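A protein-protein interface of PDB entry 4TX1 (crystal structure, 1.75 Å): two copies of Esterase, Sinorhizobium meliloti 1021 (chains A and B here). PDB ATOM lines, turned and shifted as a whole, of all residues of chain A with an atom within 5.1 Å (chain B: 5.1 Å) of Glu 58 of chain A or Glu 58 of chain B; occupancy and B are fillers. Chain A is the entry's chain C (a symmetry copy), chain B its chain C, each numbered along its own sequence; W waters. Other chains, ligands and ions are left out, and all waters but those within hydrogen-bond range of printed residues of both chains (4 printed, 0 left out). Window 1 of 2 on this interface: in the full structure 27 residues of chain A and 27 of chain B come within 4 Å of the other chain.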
ATOM      1  N   LEU A  17     -29.407  23.434  13.823  1.00  0.00           N
ATOM      2  CA  LEU A  17     -28.781  24.149  14.958  1.00  0.00           C
ATOM      3  C   LEU A  17     -28.029  25.347  14.381  1.00  0.00           C
ATOM      4  O   LEU A  17     -27.252  25.248  13.426  1.00  0.00           O
ATOM      5  CB  LEU A  17     -27.712  23.245  15.683  1.00  0.00           C
ATOM      6  CG  LEU A  17     -26.825  23.975  16.718  1.00  0.00           C
ATOM      7  CD1 LEU A  17     -27.554  24.446  17.894  1.00  0.00           C
ATOM      8  CD2 LEU A  17     -25.692  22.958  17.088  1.00  0.00           C
ATOM      9  N   CYS A  18     -28.345  26.509  14.948  1.00  0.00           N
ATOM     10  CA  CYS A  18     -27.752  27.779  14.526  1.00  0.00           C
ATOM     11  C   CYS A  18     -26.731  28.190  15.642  1.00  0.00           C
ATOM     12  O   CYS A  18     -27.175  28.579  16.738  1.00  0.00           O
ATOM     13  CB  CYS A  18     -28.819  28.835  14.531  1.00  0.00           C
ATOM     14  SG  CYS A  18     -30.001  28.495  13.129  1.00  0.00           S
ATOM     15  N   TYR A  19     -25.458  28.058  15.348  1.00  0.00           N
ATOM     16  CA  TYR A  19     -24.393  28.278  16.358  1.00  0.00           C
ATOM     17  C   TYR A  19     -23.646  29.568  16.035  1.00  0.00           C
ATOM     18  O   TYR A  19     -22.944  29.638  14.981  1.00  0.00           O
ATOM     19  CB  TYR A  19     -23.474  27.028  16.389  1.00  0.00           C
ATOM     20  CG  TYR A  19     -22.507  27.000  17.601  1.00  0.00           C
ATOM     21  CD1 TYR A  19     -22.983  26.683  18.862  1.00  0.00           C
ATOM     22  CD2 TYR A  19     -21.179  27.184  17.417  1.00  0.00           C
ATOM     23  CE1 TYR A  19     -22.144  26.626  19.956  1.00  0.00           C
ATOM     24  CE2 TYR A  19     -20.281  27.101  18.517  1.00  0.00           C
ATOM     25  CZ  TYR A  19     -20.816  26.799  19.755  1.00  0.00           C
ATOM     26  OH  TYR A  19     -19.996  26.662  20.890  1.00  0.00           O
ATOM     27  N   GLY A  20     -23.898  30.564  16.865  1.00  0.00           N
ATOM     28  CA  GLY A  20     -23.347  31.881  16.624  1.00  0.00           C
ATOM     29  C   GLY A  20     -22.991  32.717  17.803  1.00  0.00           C
ATOM     30  O   GLY A  20     -22.840  32.261  18.954  1.00  0.00           O
ATOM     31  N   THR A  24     -26.368  36.331  16.306  1.00  0.00           N
ATOM     32  CA  THR A  24     -27.383  35.268  16.397  1.00  0.00           C
ATOM     33  C   THR A  24     -28.236  35.358  17.659  1.00  0.00           C
ATOM     34  O   THR A  24     -29.442  35.148  17.603  1.00  0.00           O
ATOM     35  CB  THR A  24     -26.607  33.929  16.303  1.00  0.00           C
ATOM     36  OG1 THR A  24     -25.904  33.854  15.062  1.00  0.00           O
ATOM     37  CG2 THR A  24     -27.566  32.715  16.450  1.00  0.00           C
ATOM     38  N   ILE A  56     -33.051  25.650  16.203  1.00  0.00           N
ATOM     39  CA  ILE A  56     -32.595  25.838  17.554  1.00  0.00           C
ATOM     40  C   ILE A  56     -31.527  26.938  17.478  1.00  0.00           C
ATOM     41  O   ILE A  56     -30.595  26.837  16.673  1.00  0.00           O
ATOM     42  CB  ILE A  56     -31.908  24.549  18.070  1.00  0.00           C
ATOM     43  CG1 ILE A  56     -32.955  23.387  18.121  1.00  0.00           C
ATOM     44  CG2 ILE A  56     -31.353  24.764  19.443  1.00  0.00           C
ATOM     45  CD1 ILE A  56     -32.335  21.997  18.300  1.00  0.00           C
ATOM     46  N   ALA A  57     -31.728  27.976  18.267  1.00  0.00           N
ATOM     47  CA  ALA A  57     -30.853  29.144  18.262  1.00  0.00           C
ATOM     48  C   ALA A  57     -29.900  29.030  19.434  1.00  0.00           C
ATOM     49  O   ALA A  57     -30.336  28.995  20.570  1.00  0.00           O
ATOM     50  CB  ALA A  57     -31.723  30.420  18.462  1.00  0.00           C
ATOM     51  N   GLU A  58     -28.602  29.083  19.180  1.00  0.00           N
ATOM     52  CA  GLU A  58     -27.551  29.069  20.189  1.00  0.00           C
ATOM     53  C   GLU A  58     -26.533  30.154  19.887  1.00  0.00           C
ATOM     54  O   GLU A  58     -25.441  29.894  19.374  1.00  0.00           O
ATOM     55  CB  GLU A  58     -26.802  27.722  20.161  1.00  0.00           C
ATOM     56  CG  GLU A  58     -27.647  26.653  20.836  1.00  0.00           C
ATOM     57  CD  GLU A  58     -27.654  26.650  22.340  1.00  0.00           C
ATOM     58  OE1 GLU A  58     -26.692  27.141  23.042  1.00  0.00           O
ATOM     59  OE2 GLU A  58     -28.642  26.007  22.853  1.00  0.00           O
ATOM     60  N   GLY A  59     -26.964  31.352  20.145  1.00  0.00           N
ATOM     61  CA  GLY A  59     -26.148  32.517  19.992  1.00  0.00           C
ATOM     62  C   GLY A  59     -25.636  33.095  21.247  1.00  0.00           C
ATOM     63  O   GLY A  59     -26.403  33.382  22.180  1.00  0.00           O
ATOM     64  N   LEU A  60     -24.299  33.230  21.348  1.00  0.00           N
ATOM     65  CA  LEU A  60     -23.666  33.658  22.593  1.00  0.00           C
ATOM     66  C   LEU A  60     -22.829  34.952  22.382  1.00  0.00           C
ATOM     67  O   LEU A  60     -21.935  34.950  21.591  1.00  0.00           O
ATOM     68  CB  LEU A  60     -22.730  32.565  23.157  1.00  0.00           C
ATOM     69  CG  LEU A  60     -22.036  32.986  24.451  1.00  0.00           C
ATOM     70  CD1 LEU A  60     -22.884  33.169  25.695  1.00  0.00           C
ATOM     71  CD2 LEU A  60     -20.855  31.999  24.795  1.00  0.00           C
ATOM     72  N   ARG A  63     -18.913  35.210  21.501  1.00  0.00           N
ATOM     73  CA  ARG A  63     -18.340  33.886  21.111  1.00  0.00           C
ATOM     74  C   ARG A  63     -17.367  33.982  19.965  1.00  0.00           C
ATOM     75  O   ARG A  63     -17.631  34.582  18.910  1.00  0.00           O
ATOM     76  CB  ARG A  63     -19.436  32.856  20.745  1.00  0.00           C
ATOM     77  CG  ARG A  63     -18.860  31.539  20.272  1.00  0.00           C
ATOM     78  CD  ARG A  63     -20.017  30.550  20.025  1.00  0.00           C
ATOM     79  NE  ARG A  63     -20.522  30.048  21.278  1.00  0.00           N
ATOM     80  CZ  ARG A  63     -21.741  29.608  21.540  1.00  0.00           C
ATOM     81  NH1 ARG A  63     -22.783  29.869  20.741  1.00  0.00           N
ATOM     82  NH2 ARG A  63     -21.937  28.948  22.670  1.00  0.00           N
ATOM     83  N   VAL A  85     -23.137  21.537  23.249  1.00  0.00           N
ATOM     84  CA  VAL A  85     -24.302  22.023  22.490  1.00  0.00           C
ATOM     85  C   VAL A  85     -24.792  20.962  21.459  1.00  0.00           C
ATOM     86  O   VAL A  85     -25.975  20.666  21.400  1.00  0.00           O
ATOM     87  CB  VAL A  85     -23.958  23.360  21.800  1.00  0.00           C
ATOM     88  CG1 VAL A  85     -25.087  23.897  20.916  1.00  0.00           C
ATOM     89  CG2 VAL A  85     -23.711  24.408  22.861  1.00  0.00           C
ATOM     90  N   THR A  88     -26.580  18.238  23.380  1.00  0.00           N
ATOM     91  CA  THR A  88     -27.844  18.710  23.916  1.00  0.00           C
ATOM     92  C   THR A  88     -28.934  18.637  22.896  1.00  0.00           C
ATOM     93  O   THR A  88     -30.088  18.424  23.256  1.00  0.00           O
ATOM     94  CB  THR A  88     -27.656  20.155  24.410  1.00  0.00           C
ATOM     95  OG1 THR A  88     -26.725  20.176  25.521  1.00  0.00           O
ATOM     96  CG2 THR A  88     -28.996  20.803  24.888  1.00  0.00           C
ATOM     97  N   HIS A  89     -28.560  18.934  21.668  1.00  0.00           N
ATOM     98  CA  HIS A  89     -29.573  19.102  20.591  1.00  0.00           C
ATOM     99  C   HIS A  89     -29.622  18.023  19.535  1.00  0.00           C
ATOM    100  O   HIS A  89     -30.499  18.052  18.655  1.00  0.00           O
ATOM    101  CB  HIS A  89     -29.420  20.508  19.971  1.00  0.00           C
ATOM    102  CG  HIS A  89     -29.668  21.593  20.928  1.00  0.00           C
ATOM    103  ND1 HIS A  89     -30.832  21.713  21.652  1.00  0.00           N
ATOM    104  CD2 HIS A  89     -28.852  22.602  21.365  1.00  0.00           C
ATOM    105  CE1 HIS A  89     -30.746  22.741  22.464  1.00  0.00           C
ATOM    106  NE2 HIS A  89     -29.549  23.298  22.306  1.00  0.00           N
ATOM    107  N   LEU B  17     -36.506  28.821  30.624  1.00  0.00           N
ATOM    108  CA  LEU B  17     -35.383  27.917  30.288  1.00  0.00           C
ATOM    109  C   LEU B  17     -35.547  26.655  31.134  1.00  0.00           C
ATOM    110  O   LEU B  17     -35.749  26.691  32.352  1.00  0.00           O
ATOM    111  CB  LEU B  17     -33.997  28.555  30.685  1.00  0.00           C
ATOM    112  CG  LEU B  17     -32.785  27.597  30.611  1.00  0.00           C
ATOM    113  CD1 LEU B  17     -32.452  27.170  29.253  1.00  0.00           C
ATOM    114  CD2 LEU B  17     -31.604  28.364  31.299  1.00  0.00           C
ATOM    115  N   CYS B  18     -35.530  25.525  30.430  1.00  0.00           N
ATOM    116  CA  CYS B  18     -35.693  24.209  31.049  1.00  0.00           C
ATOM    117  C   CYS B  18     -34.278  23.534  31.047  1.00  0.00           C
ATOM    118  O   CYS B  18     -33.809  23.142  29.962  1.00  0.00           O
ATOM    119  CB  CYS B  18     -36.558  23.362  30.161  1.00  0.00           C
ATOM    120  SG  CYS B  18     -38.301  24.018  30.225  1.00  0.00           S
ATOM    121  N   TYR B  19     -33.663  23.462  32.205  1.00  0.00           N
ATOM    122  CA  TYR B  19     -32.264  22.975  32.320  1.00  0.00           C
ATOM    123  C   TYR B  19     -32.258  21.604  32.988  1.00  0.00           C
ATOM    124  O   TYR B  19     -32.613  21.496  34.201  1.00  0.00           O
ATOM    125  CB  TYR B  19     -31.433  24.036  33.090  1.00  0.00           C
ATOM    126  CG  TYR B  19     -29.903  23.794  33.019  1.00  0.00           C
ATOM    127  CD1 TYR B  19     -29.207  24.087  31.859  1.00  0.00           C
ATOM    128  CD2 TYR B  19     -29.226  23.393  34.120  1.00  0.00           C
ATOM    129  CE1 TYR B  19     -27.841  23.905  31.774  1.00  0.00           C
ATOM    130  CE2 TYR B  19     -27.814  23.226  34.077  1.00  0.00           C
ATOM    131  CZ  TYR B  19     -27.175  23.517  32.887  1.00  0.00           C
ATOM    132  OH  TYR B  19     -25.777  23.414  32.765  1.00  0.00           O
ATOM    133  N   GLY B  20     -31.974  20.605  32.173  1.00  0.00           N
ATOM    134  CA  GLY B  20     -32.036  19.235  32.637  1.00  0.00           C
ATOM    135  C   GLY B  20     -31.074  18.256  32.061  1.00  0.00           C
ATOM    136  O   GLY B  20     -30.035  18.583  31.454  1.00  0.00           O
ATOM    137  N   THR B  24     -34.992  15.431  30.222  1.00  0.00           N
ATOM    138  CA  THR B  24     -35.383  16.647  29.489  1.00  0.00           C
ATOM    139  C   THR B  24     -34.998  16.607  28.013  1.00  0.00           C
ATOM    140  O   THR B  24     -35.773  17.031  27.163  1.00  0.00           O
ATOM    141  CB  THR B  24     -34.721  17.830  30.240  1.00  0.00           C
ATOM    142  OG1 THR B  24     -35.188  17.879  31.589  1.00  0.00           O
ATOM    143  CG2 THR B  24     -35.008  19.178  29.523  1.00  0.00           C
ATOM    144  N   ILE B  56     -37.442  27.100  26.150  1.00  0.00           N
ATOM    145  CA  ILE B  56     -36.172  26.725  25.588  1.00  0.00           C
ATOM    146  C   ILE B  56     -35.742  25.463  26.349  1.00  0.00           C
ATOM    147  O   ILE B  56     -35.733  25.462  27.585  1.00  0.00           O
ATOM    148  CB  ILE B  56     -35.119  27.826  25.868  1.00  0.00           C
ATOM    149  CG1 ILE B  56     -35.543  29.147  25.144  1.00  0.00           C
ATOM    150  CG2 ILE B  56     -33.774  27.406  25.363  1.00  0.00           C
ATOM    151  CD1 ILE B  56     -34.767  30.386  25.604  1.00  0.00           C
ATOM    152  N   ALA B  57     -35.464  24.417  25.595  1.00  0.00           N
ATOM    153  CA  ALA B  57     -35.116  23.117  26.160  1.00  0.00           C
ATOM    154  C   ALA B  57     -33.609  22.964  26.112  1.00  0.00           C
ATOM    155  O   ALA B  57     -33.030  22.984  25.041  1.00  0.00           O
ATOM    156  CB  ALA B  57     -35.747  22.003  25.273  1.00  0.00           C
ATOM    157  N   GLU B  58     -32.981  22.703  27.247  1.00  0.00           N
ATOM    158  CA  GLU B  58     -31.552  22.449  27.372  1.00  0.00           C
ATOM    159  C   GLU B  58     -31.320  21.229  28.245  1.00  0.00           C
ATOM    160  O   GLU B  58     -30.961  21.331  29.421  1.00  0.00           O
ATOM    161  CB  GLU B  58     -30.855  23.639  28.060  1.00  0.00           C
ATOM    162  CG  GLU B  58     -30.700  24.784  27.071  1.00  0.00           C
ATOM    163  CD  GLU B  58     -29.577  24.665  26.076  1.00  0.00           C
ATOM    164  OE1 GLU B  58     -28.524  23.957  26.295  1.00  0.00           O
ATOM    165  OE2 GLU B  58     -29.710  25.430  25.051  1.00  0.00           O
ATOM    166  N   GLY B  59     -31.614  20.109  27.656  1.00  0.00           N
ATOM    167  CA  GLY B  59     -31.414  18.835  28.273  1.00  0.00           C
ATOM    168  C   GLY B  59     -30.250  18.075  27.784  1.00  0.00           C
ATOM    169  O   GLY B  59     -30.092  17.854  26.573  1.00  0.00           O
ATOM    170  N   LEU B  60     -29.344  17.697  28.708  1.00  0.00           N
ATOM    171  CA  LEU B  60     -28.084  17.065  28.329  1.00  0.00           C
ATOM    172  C   LEU B  60     -27.938  15.664  28.990  1.00  0.00           C
ATOM    173  O   LEU B  60     -27.959  15.572  30.180  1.00  0.00           O
ATOM    174  CB  LEU B  60     -26.870  17.925  28.748  1.00  0.00           C
ATOM    175  CG  LEU B  60     -25.533  17.284  28.383  1.00  0.00           C
ATOM    176  CD1 LEU B  60     -25.175  17.154  26.915  1.00  0.00           C
ATOM    177  CD2 LEU B  60     -24.346  18.015  29.121  1.00  0.00           C
ATOM    178  N   ARG B  63     -26.143  14.788  32.482  1.00  0.00           N
ATOM    179  CA  ARG B  63     -25.834  16.017  33.275  1.00  0.00           C
ATOM    180  C   ARG B  63     -26.089  15.843  34.750  1.00  0.00           C
ATOM    181  O   ARG B  63     -27.154  15.387  35.197  1.00  0.00           O
ATOM    182  CB  ARG B  63     -26.626  17.251  32.778  1.00  0.00           C
ATOM    183  CG  ARG B  63     -26.379  18.479  33.627  1.00  0.00           C
ATOM    184  CD  ARG B  63     -27.128  19.675  33.003  1.00  0.00           C
ATOM    185  NE  ARG B  63     -26.422  20.155  31.842  1.00  0.00           N
ATOM    186  CZ  ARG B  63     -26.926  20.781  30.792  1.00  0.00           C
ATOM    187  NH1 ARG B  63     -28.236  20.775  30.516  1.00  0.00           N
ATOM    188  NH2 ARG B  63     -26.088  21.372  29.955  1.00  0.00           N
ATOM    189  N   VAL B  85     -25.107  28.807  29.277  1.00  0.00           N
ATOM    190  CA  VAL B  85     -26.505  28.597  28.863  1.00  0.00           C
ATOM    191  C   VAL B  85     -27.402  29.808  29.261  1.00  0.00           C
ATOM    192  O   VAL B  85     -28.148  30.313  28.437  1.00  0.00           O
ATOM    193  CB  VAL B  85     -27.039  27.281  29.466  1.00  0.00           C
ATOM    194  CG1 VAL B  85     -28.517  27.026  29.158  1.00  0.00           C
ATOM    195  CG2 VAL B  85     -26.272  26.124  28.869  1.00  0.00           C
ATOM    196  N   THR B  88     -26.622  32.641  26.879  1.00  0.00           N
ATOM    197  CA  THR B  88     -27.110  32.359  25.542  1.00  0.00           C
ATOM    198  C   THR B  88     -28.557  32.707  25.401  1.00  0.00           C
ATOM    199  O   THR B  88     -28.986  33.091  24.318  1.00  0.00           O
ATOM    200  CB  THR B  88     -26.876  30.868  25.240  1.00  0.00           C
ATOM    201  OG1 THR B  88     -25.454  30.593  25.205  1.00  0.00           O
ATOM    202  CG2 THR B  88     -27.489  30.432  23.869  1.00  0.00           C
ATOM    203  N   HIS B  89     -29.291  32.448  26.465  1.00  0.00           N
ATOM    204  CA  HIS B  89     -30.774  32.551  26.401  1.00  0.00           C
ATOM    205  C   HIS B  89     -31.405  33.703  27.146  1.00  0.00           C
ATOM    206  O   HIS B  89     -32.630  33.902  27.065  1.00  0.00           O
ATOM    207  CB  HIS B  89     -31.390  31.195  26.810  1.00  0.00           C
ATOM    208  CG  HIS B  89     -31.024  30.097  25.905  1.00  0.00           C
ATOM    209  ND1 HIS B  89     -31.246  30.127  24.548  1.00  0.00           N
ATOM    210  CD2 HIS B  89     -30.354  28.927  26.148  1.00  0.00           C
ATOM    211  CE1 HIS B  89     -30.765  29.038  23.996  1.00  0.00           C
ATOM    212  NE2 HIS B  89     -30.218  28.292  24.951  1.00  0.00           N
HETATM  213  O   HOH W   1     -24.706  28.774  23.097  1.00  0.00           O
HETATM  214  O   HOH W   2     -32.354  19.444  24.954  1.00  0.00           O
HETATM  215  O   HOH W   3     -27.504  21.998  27.615  1.00  0.00           O
HETATM  216  O   HOH W   4     -29.341  32.355  21.421  1.00  0.00           O
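Of the 14 printed residues of chain A, 6 touch a printed residue of chain B.
Printed residues of chain B that touch a printed residue of chain A: Ala 57, Glu 58, Gly 59, Leu 60, Thr 88 and His 89.
Among the printed residues, no Asp or Glu carboxylate lies within 4 Å of a Lys or Arg side-chain nitrogen of the other chain.
Water W3 lies within hydrogen-bond range of the side-chain carboxylate (OE1) of Glu 58 of chain B (2.6 Å), the guanidinium group (NH2) of Arg 63 of chain B (2.8 Å) and the side-chain hydroxyl (OG1) of Thr 88 of chain A (2.9 Å).
Water W1 lies within hydrogen-bond range of OE1 of Glu 58 of chain A (2.6 Å), NH2 of Arg 63 of chain A (2.8 Å) and OG1 of Thr 88 of chain B (2.9 Å).
Water W4 bridges N of Gly 59 of chain A (2.9 Å) and O of Thr 88 of chain B (3.0 Å).
Water W2 bridges N of Gly 59 of chain B and O of Thr 88 of chain A.
O of Ala 57 of chain A touches CE1 of His 89 of chain B (3.5 Å).
Thr 88 of chain B touches Glu 58 of chain A.
CD1 of Leu 60 of chain A touches OG1 of Thr 88 of chain B (3.7 Å).
CG2 of Thr 88 of chain A touches OE1 of Glu 58 of chain B, 3.5 Å away.
OG1 of Thr 88 of chain A touches CD1 of Leu 60 of chain B, at 3.7 Å.
His 89 of chain A touches Ala 57 of chain B (CE1 to O, 3.5 Å).
Of chain B, only Glu 58 (2.5 Å), Thr 88 (3.5 Å) and His 89 (3.5 Å) come within 4 Å of Glu 58 of chain A.
Of chain A, only Glu 58, Thr 88 and His 89 come within 4 Å of Glu 58 of chain B.
Printed residues of chain A within 4 Å of Gly 59 of chain B: Thr 88 (3.4 Å).
Of the printed residues of chain A, His 89 of chain B touches Ala 57 (3.5 Å) and Glu 58 (3.5 Å).
Printed residues of chain A within 4 Å of Ala 57 of chain B: His 89.
Arg 63 of chain B touches none of the printed residues of chain A.
The nearest printed residue of chain B that does not touch Glu 58 of chain A is Ala 57 of chain B (5.8 Å).
A ring nitrogen (NE2) of His 89 of chain B sits at hydrogen-bond distance from the side-chain carboxylate (OE2) of Glu 58 of chain A.
The backbone carbonyl oxygen of Gly 59 of chain A lies close to the backbone carbonyl oxygen of Thr 88 of chain B (3.4 Å).
O of Thr 88 of chain A sits close to O of Gly 59 of chain B (3.4 Å).
OE2 of Glu 58 of chain B sits close to OE2 of Glu 58 of chain A (2.5 Å).
A ring nitrogen (NE2) of His 89 of chain A sits at hydrogen-bond distance from the side-chain carboxylate (OE2) of Glu 58 of chain B (3.5 Å).
NH1 of Arg 63 of chain B lies within hydrogen-bond range of O of Glu 58 of chain B (3.0 Å).
The backbone NH of Leu 60 of chain B sits at hydrogen-bond distance from the backbone carbonyl oxygen of Gly 20 of chain B (3.0 Å).
N of Leu 60 of chain A sits at hydrogen-bond distance from O of Gly 20 of chain A (3.0 Å).
N of Gly 20 of chain B sits at hydrogen-bond distance from O of Glu 58 of chain B, 3.0 Å away.
O of Glu 58 of chain A sits at hydrogen-bond distance from NH1 of Arg 63 of chain A.
OE2 of Glu 58 of chain A sits at hydrogen-bond distance from NE2 of His 89 of chain A (2.9 Å).
Glu 58 of chain A touches its own counterpart, Glu 58 of chain B.
Glu 58 of chain A touches Thr 88 of chain B, and with the chains exchanged Thr 88 of chain A touches Glu 58 of chain B.
Glu 58 of chain A touches His 89 of chain B, and with the chains exchanged His 89 of chain A touches Glu 58 of chain B.
Leu 60 of chain A touches Thr 88 of chain B, and with the chains exchanged Thr 88 of chain A touches Leu 60 of chain B.
14 positions are printed for both chains.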
